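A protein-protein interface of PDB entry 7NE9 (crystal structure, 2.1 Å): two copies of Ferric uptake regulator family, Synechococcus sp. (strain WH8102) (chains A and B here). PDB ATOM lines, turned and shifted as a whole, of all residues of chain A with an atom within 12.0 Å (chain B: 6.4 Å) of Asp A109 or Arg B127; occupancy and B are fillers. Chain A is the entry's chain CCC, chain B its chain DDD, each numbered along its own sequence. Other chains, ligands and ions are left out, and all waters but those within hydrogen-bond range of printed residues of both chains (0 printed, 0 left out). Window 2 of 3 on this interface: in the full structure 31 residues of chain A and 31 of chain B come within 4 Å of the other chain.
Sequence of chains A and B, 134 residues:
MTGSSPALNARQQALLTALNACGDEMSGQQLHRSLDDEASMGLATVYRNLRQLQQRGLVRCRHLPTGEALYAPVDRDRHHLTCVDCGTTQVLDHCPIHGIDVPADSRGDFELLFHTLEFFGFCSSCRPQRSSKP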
ATOM      1  N   PRO A   6      22.683  -5.436  -3.905  1.00  0.00           N
ATOM      2  CA  PRO A   6      21.589  -6.427  -3.753  1.00  0.00           C
ATOM      3  C   PRO A   6      21.798  -7.678  -4.632  1.00  0.00           C
ATOM      4  O   PRO A   6      22.941  -7.992  -4.920  1.00  0.00           O
ATOM      5  CB  PRO A   6      20.334  -5.627  -4.154  1.00  0.00           C
ATOM      6  CG  PRO A   6      20.628  -4.236  -3.633  1.00  0.00           C
ATOM      7  CD  PRO A   6      22.139  -4.087  -3.684  1.00  0.00           C
ATOM      8  N   GLN A  54      18.849  -1.499 -16.265  1.00  0.00           N
ATOM      9  CA  GLN A  54      19.612  -0.367 -16.845  1.00  0.00           C
ATOM     10  C   GLN A  54      20.211   0.455 -15.708  1.00  0.00           C
ATOM     11  O   GLN A  54      21.378   0.844 -15.816  1.00  0.00           O
ATOM     12  CB  GLN A  54      18.723   0.512 -17.718  1.00  0.00           C
ATOM     13  CG  GLN A  54      18.565  -0.020 -19.128  1.00  0.00           C
ATOM     14  CD  GLN A  54      17.541   0.790 -19.885  1.00  0.00           C
ATOM     15  OE1 GLN A  54      16.333   0.599 -19.715  1.00  0.00           O
ATOM     16  NE2 GLN A  54      18.025   1.724 -20.685  1.00  0.00           N
ATOM     17  N   GLN A  55      19.427   0.714 -14.664  1.00  0.00           N
ATOM     18  CA  GLN A  55      19.838   1.549 -13.510  1.00  0.00           C
ATOM     19  C   GLN A  55      20.972   0.854 -12.761  1.00  0.00           C
ATOM     20  O   GLN A  55      21.812   1.571 -12.193  1.00  0.00           O
ATOM     21  CB  GLN A  55      18.655   1.810 -12.582  1.00  0.00           C
ATOM     22  CG  GLN A  55      17.665   2.810 -13.146  1.00  0.00           C
ATOM     23  CD  GLN A  55      16.620   3.117 -12.109  1.00  0.00           C
ATOM     24  OE1 GLN A  55      15.848   2.249 -11.736  1.00  0.00           O
ATOM     25  NE2 GLN A  55      16.623   4.340 -11.596  1.00  0.00           N
ATOM     26  N   ARG A  56      21.011  -0.479 -12.784  1.00  0.00           N
ATOM     27  CA  ARG A  56      22.098  -1.281 -12.172  1.00  0.00           C
ATOM     28  C   ARG A  56      23.270  -1.438 -13.144  1.00  0.00           C
ATOM     29  O   ARG A  56      24.229  -2.099 -12.782  1.00  0.00           O
ATOM     30  CB  ARG A  56      21.564  -2.642 -11.734  1.00  0.00           C
ATOM     31  CG  ARG A  56      20.488  -2.514 -10.667  1.00  0.00           C
ATOM     32  CD  ARG A  56      19.880  -3.834 -10.276  1.00  0.00           C
ATOM     33  NE  ARG A  56      20.820  -4.492  -9.392  1.00  0.00           N
ATOM     34  CZ  ARG A  56      20.492  -5.363  -8.456  1.00  0.00           C
ATOM     35  NH1 ARG A  56      19.220  -5.691  -8.276  1.00  0.00           N
ATOM     36  NH2 ARG A  56      21.445  -5.871  -7.692  1.00  0.00           N
ATOM     37  N   GLY A  57      23.192  -0.872 -14.344  1.00  0.00           N
ATOM     38  CA  GLY A  57      24.286  -0.924 -15.331  1.00  0.00           C
ATOM     39  C   GLY A  57      24.478  -2.318 -15.914  1.00  0.00           C
ATOM     40  O   GLY A  57      25.580  -2.583 -16.365  1.00  0.00           O
ATOM     41  N   LEU A  58      23.448  -3.165 -15.957  1.00  0.00           N
ATOM     42  CA  LEU A  58      23.570  -4.557 -16.478  1.00  0.00           C
ATOM     43  C   LEU A  58      23.051  -4.627 -17.916  1.00  0.00           C
ATOM     44  O   LEU A  58      23.386  -5.609 -18.602  1.00  0.00           O
ATOM     45  CB  LEU A  58      22.788  -5.523 -15.578  1.00  0.00           C
ATOM     46  CG  LEU A  58      23.215  -5.571 -14.117  1.00  0.00           C
ATOM     47  CD1 LEU A  58      22.267  -6.427 -13.292  1.00  0.00           C
ATOM     48  CD2 LEU A  58      24.640  -6.077 -14.002  1.00  0.00           C
ATOM     49  N   VAL A 102      38.405   9.311 -21.815  1.00  0.00           N
ATOM     50  CA  VAL A 102      37.196  10.066 -21.342  1.00  0.00           C
ATOM     51  C   VAL A 102      36.948   9.680 -19.883  1.00  0.00           C
ATOM     52  O   VAL A 102      37.056  10.596 -19.082  1.00  0.00           O
ATOM     53  CB  VAL A 102      35.883   9.861 -22.126  1.00  0.00           C
ATOM     54  CG1 VAL A 102      35.630  11.003 -23.093  1.00  0.00           C
ATOM     55  CG2 VAL A 102      35.799   8.516 -22.826  1.00  0.00           C
ATOM     56  N   GLY A 108      36.747  12.780 -12.481  1.00  0.00           N
ATOM     57  CA  GLY A 108      36.452  13.337 -11.143  1.00  0.00           C
ATOM     58  C   GLY A 108      35.698  12.341 -10.279  1.00  0.00           C
ATOM     59  O   GLY A 108      36.374  11.674  -9.458  1.00  0.00           O
ATOM     60  N   ASP A 109      34.363  12.252 -10.453  1.00  0.00           N
ATOM     61  CA  ASP A 109      33.499  11.199  -9.854  1.00  0.00           C
ATOM     62  C   ASP A 109      32.259  10.966 -10.742  1.00  0.00           C
ATOM     63  O   ASP A 109      31.125  10.962 -10.225  1.00  0.00           O
ATOM     64  CB  ASP A 109      33.165  11.513  -8.393  1.00  0.00           C
ATOM     65  CG  ASP A 109      32.787  10.283  -7.576  1.00  0.00           C
ATOM     66  OD1 ASP A 109      32.639   9.196  -8.180  1.00  0.00           O
ATOM     67  OD2 ASP A 109      32.644  10.418  -6.339  1.00  0.00           O
ATOM     68  N   PHE A 110      32.497  10.714 -12.030  1.00  0.00           N
ATOM     69  CA  PHE A 110      31.606   9.976 -12.954  1.00  0.00           C
ATOM     70  C   PHE A 110      32.276   8.629 -13.273  1.00  0.00           C
ATOM     71  O   PHE A 110      33.436   8.630 -13.733  1.00  0.00           O
ATOM     72  CB  PHE A 110      31.359  10.821 -14.202  1.00  0.00           C
ATOM     73  CG  PHE A 110      30.350  10.237 -15.153  1.00  0.00           C
ATOM     74  CD1 PHE A 110      28.994  10.480 -14.991  1.00  0.00           C
ATOM     75  CD2 PHE A 110      30.760   9.431 -16.206  1.00  0.00           C
ATOM     76  CE1 PHE A 110      28.065   9.923 -15.852  1.00  0.00           C
ATOM     77  CE2 PHE A 110      29.832   8.869 -17.070  1.00  0.00           C
ATOM     78  CZ  PHE A 110      28.488   9.126 -16.895  1.00  0.00           C
ATOM     79  N   GLU A 111      31.593   7.510 -13.012  1.00  0.00           N
ATOM     80  CA  GLU A 111      32.136   6.156 -13.313  1.00  0.00           C
ATOM     81  C   GLU A 111      31.599   5.704 -14.674  1.00  0.00           C
ATOM     82  O   GLU A 111      30.391   5.412 -14.764  1.00  0.00           O
ATOM     83  CB  GLU A 111      31.788   5.139 -12.225  1.00  0.00           C
ATOM     84  CG  GLU A 111      32.455   3.782 -12.441  1.00  0.00           C
ATOM     85  CD  GLU A 111      32.061   2.689 -11.461  1.00  0.00           C
ATOM     86  OE1 GLU A 111      31.960   3.001 -10.243  1.00  0.00           O
ATOM     87  OE2 GLU A 111      31.841   1.534 -11.915  1.00  0.00           O
ATOM     88  N   LEU A 112      32.470   5.614 -15.682  1.00  0.00           N
ATOM     89  CA  LEU A 112      32.133   5.224 -17.071  1.00  0.00           C
ATOM     90  C   LEU A 112      31.828   3.720 -17.162  1.00  0.00           C
ATOM     91  O   LEU A 112      32.624   2.935 -16.657  1.00  0.00           O
ATOM     92  CB  LEU A 112      33.331   5.583 -17.944  1.00  0.00           C
ATOM     93  CG  LEU A 112      33.129   5.417 -19.445  1.00  0.00           C
ATOM     94  CD1 LEU A 112      32.106   6.427 -19.952  1.00  0.00           C
ATOM     95  CD2 LEU A 112      34.462   5.562 -20.172  1.00  0.00           C
ATOM     96  N   LEU A 113      30.725   3.344 -17.808  1.00  0.00           N
ATOM     97  CA  LEU A 113      30.322   1.930 -18.011  1.00  0.00           C
ATOM     98  C   LEU A 113      30.398   1.565 -19.492  1.00  0.00           C
ATOM     99  O   LEU A 113      30.890   0.476 -19.794  1.00  0.00           O
ATOM    100  CB  LEU A 113      28.894   1.737 -17.506  1.00  0.00           C
ATOM    101  CG  LEU A 113      28.709   1.731 -15.993  1.00  0.00           C
ATOM    102  CD1 LEU A 113      27.250   1.479 -15.665  1.00  0.00           C
ATOM    103  CD2 LEU A 113      29.569   0.677 -15.302  1.00  0.00           C
ATOM    104  N   ASP B  85      21.444   5.677 -13.855  1.00  0.00           N
ATOM    105  CA  ASP B  85      20.554   5.570 -12.670  1.00  0.00           C
ATOM    106  C   ASP B  85      19.598   6.772 -12.644  1.00  0.00           C
ATOM    107  O   ASP B  85      18.410   6.565 -12.892  1.00  0.00           O
ATOM    108  CB  ASP B  85      21.368   5.408 -11.388  1.00  0.00           C
ATOM    109  CG  ASP B  85      20.524   4.946 -10.210  1.00  0.00           C
ATOM    110  OD1 ASP B  85      19.292   4.950 -10.330  1.00  0.00           O
ATOM    111  OD2 ASP B  85      21.121   4.602  -9.172  1.00  0.00           O
ATOM    112  N   PHE B 122      27.789   5.962 -13.970  1.00  0.00           N
ATOM    113  CA  PHE B 122      27.171   6.368 -12.694  1.00  0.00           C
ATOM    114  C   PHE B 122      27.761   7.713 -12.287  1.00  0.00           C
ATOM    115  O   PHE B 122      29.001   7.836 -12.280  1.00  0.00           O
ATOM    116  CB  PHE B 122      27.444   5.338 -11.600  1.00  0.00           C
ATOM    117  CG  PHE B 122      26.897   3.960 -11.843  1.00  0.00           C
ATOM    118  CD1 PHE B 122      25.532   3.753 -11.915  1.00  0.00           C
ATOM    119  CD2 PHE B 122      27.740   2.859 -11.923  1.00  0.00           C
ATOM    120  CE1 PHE B 122      25.020   2.473 -12.084  1.00  0.00           C
ATOM    121  CE2 PHE B 122      27.228   1.583 -12.100  1.00  0.00           C
ATOM    122  CZ  PHE B 122      25.870   1.392 -12.181  1.00  0.00           C
ATOM    123  N   CYS B 123      26.907   8.671 -11.931  1.00  0.00           N
ATOM    124  CA  CYS B 123      27.324   9.947 -11.310  1.00  0.00           C
ATOM    125  C   CYS B 123      27.766   9.679  -9.863  1.00  0.00           C
ATOM    126  O   CYS B 123      27.529   8.552  -9.366  1.00  0.00           O
ATOM    127  CB  CYS B 123      26.201  10.974 -11.409  1.00  0.00           C
ATOM    128  SG  CYS B 123      24.903  10.754 -10.166  1.00  0.00           S
ATOM    129  N   SER B 124      28.352  10.691  -9.208  1.00  0.00           N
ATOM    130  CA  SER B 124      28.912  10.630  -7.835  1.00  0.00           C
ATOM    131  C   SER B 124      27.871  10.097  -6.850  1.00  0.00           C
ATOM    132  O   SER B 124      28.224   9.210  -6.062  1.00  0.00           O
ATOM    133  CB  SER B 124      29.457  11.979  -7.413  1.00  0.00           C
ATOM    134  OG  SER B 124      28.435  12.958  -7.297  1.00  0.00           O
ATOM    135  N   SER B 125      26.643  10.617  -6.883  1.00  0.00           N
ATOM    136  CA  SER B 125      25.521  10.187  -6.005  1.00  0.00           C
ATOM    137  C   SER B 125      25.187   8.691  -6.186  1.00  0.00           C
ATOM    138  O   SER B 125      24.826   8.072  -5.176  1.00  0.00           O
ATOM    139  CB  SER B 125      24.287  11.012  -6.245  1.00  0.00           C
ATOM    140  OG  SER B 125      24.611  12.383  -6.347  1.00  0.00           O
ATOM    141  N   CYS B 126      25.284   8.130  -7.399  1.00  0.00           N
ATOM    142  CA  CYS B 126      24.534   6.903  -7.768  1.00  0.00           C
ATOM    143  C   CYS B 126      25.301   5.578  -7.625  1.00  0.00           C
ATOM    144  O   CYS B 126      24.564   4.581  -7.501  1.00  0.00           O
ATOM    145  CB  CYS B 126      23.945   7.002  -9.170  1.00  0.00           C
ATOM    146  SG  CYS B 126      22.466   8.052  -9.251  1.00  0.00           S
ATOM    147  N   ARG B 127      26.638   5.506  -7.631  1.00  0.00           N
ATOM    148  CA  ARG B 127      27.343   4.176  -7.658  1.00  0.00           C
ATOM    149  C   ARG B 127      27.175   3.439  -6.321  1.00  0.00           C
ATOM    150  O   ARG B 127      27.504   4.004  -5.282  1.00  0.00           O
ATOM    151  CB  ARG B 127      28.832   4.312  -7.989  1.00  0.00           C
ATOM    152  CG  ARG B 127      29.547   5.381  -7.189  1.00  0.00           C
ATOM    153  CD  ARG B 127      29.892   6.576  -8.054  1.00  0.00           C
ATOM    154  NE  ARG B 127      31.063   6.418  -8.911  1.00  0.00           N
ATOM    155  CZ  ARG B 127      32.320   6.256  -8.488  1.00  0.00           C
ATOM    156  NH1 ARG B 127      32.605   6.197  -7.196  1.00  0.00           N
ATOM    157  NH2 ARG B 127      33.305   6.155  -9.365  1.00  0.00           N
ATOM    158  N   PRO B 128      26.612   2.197  -6.291  1.00  0.00           N
ATOM    159  CA  PRO B 128      26.310   1.506  -5.033  1.00  0.00           C
ATOM    160  C   PRO B 128      27.472   0.633  -4.544  1.00  0.00           C
ATOM    161  O   PRO B 128      28.357   1.146  -3.868  1.00  0.00           O
ATOM    162  CB  PRO B 128      25.089   0.633  -5.381  1.00  0.00           C
ATOM    163  CG  PRO B 128      25.269   0.316  -6.858  1.00  0.00           C
ATOM    164  CD  PRO B 128      26.107   1.440  -7.453  1.00  0.00           C
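SG of Cys B126 sits close to OD2 of Asp B85 (3.7 Å). N of Ser B125 sits close to SG of Cys B123 (3.7 Å).
Printed residues of chain B within 4 Å of Gln A55: Asp B85 (3.0 Å) and Phe B122 (3.3 Å). Asp A109 touches just these residues of chain B: Cys B123, Ser B124 and Arg B127. Of the printed residues of chain B, Phe A110 touches Phe B122 (3.4 Å). Of the printed residues of chain B, Glu A111 touches Phe B122 (2.7 Å) and Arg B127 (3.4 Å). Of the printed residues of chain B, Leu A113 touches Phe B122. Phe B122 touches just these residues of chain A: Gln A55 (3.3 Å), Arg A56 (3.9 Å), Phe A110 (3.4 Å), Glu A111 (2.7 Å) and Leu A113 (3.6 Å). Of chain A, only Asp A109 (3.0 Å) comes within 4 Å of Ser B124. No residue of chain A comes within 4 Å of Ser B125. No residue of chain A comes within 4 Å of Cys B126. Of chain A, only Asp A109 (3.0 Å) and Glu A111 (3.4 Å) come within 4 Å of Arg B127. The nearest residue of chain A that does not touch Arg B127 is Phe A110 (4.7 Å).
CE1 of Phe B122 touches O of Gln A55, 3.3 Å away. Phe B122 touches Arg A56 (CZ to O, 3.9 Å). O of Asp A109 touches C of Cys B123 (3.6 Å). Phe B122 touches Phe A110. Leu A113 touches Phe B122 (CD1 to CE2, 3.6 Å).
OE1 of Glu A111 lies within salt-bridge range of NH2 of Arg B127 (3.5 Å). The backbone carbonyl oxygen of Phe B122 lies within hydrogen-bond range of the backbone NH of Glu A111, at 2.7 Å. The side-chain carboxylate (OD1) of Asp B85 sits at hydrogen-bond distance from the side-chain amide nitrogen (NE2) of Gln A55. The backbone carbonyl oxygen of Asp A109 lies within hydrogen-bond range of the backbone NH of Ser B124. NH1 of Arg B127 is in salt-bridge range of OD1 of Asp A109, at 3.2 Å.
No position is printed for both chains. Of the 10 pairs that touch across the chains among the printed residues, none has its exchanged pair printed and touching as well.
Hydrophobic or aromatic side chains of chain A that line the printed part of chain B: Phe A110 and Leu A113. Of the 8 printed residues of chain B, 5 touch a printed residue of chain A. Among the printed residues, Asp or Glu carboxylates within 4 Å of a Lys or Arg side-chain nitrogen of the other chain: Asp A109 with Arg B127 (3.2 Å) and Glu A111 with Arg B127 (3.5 Å).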
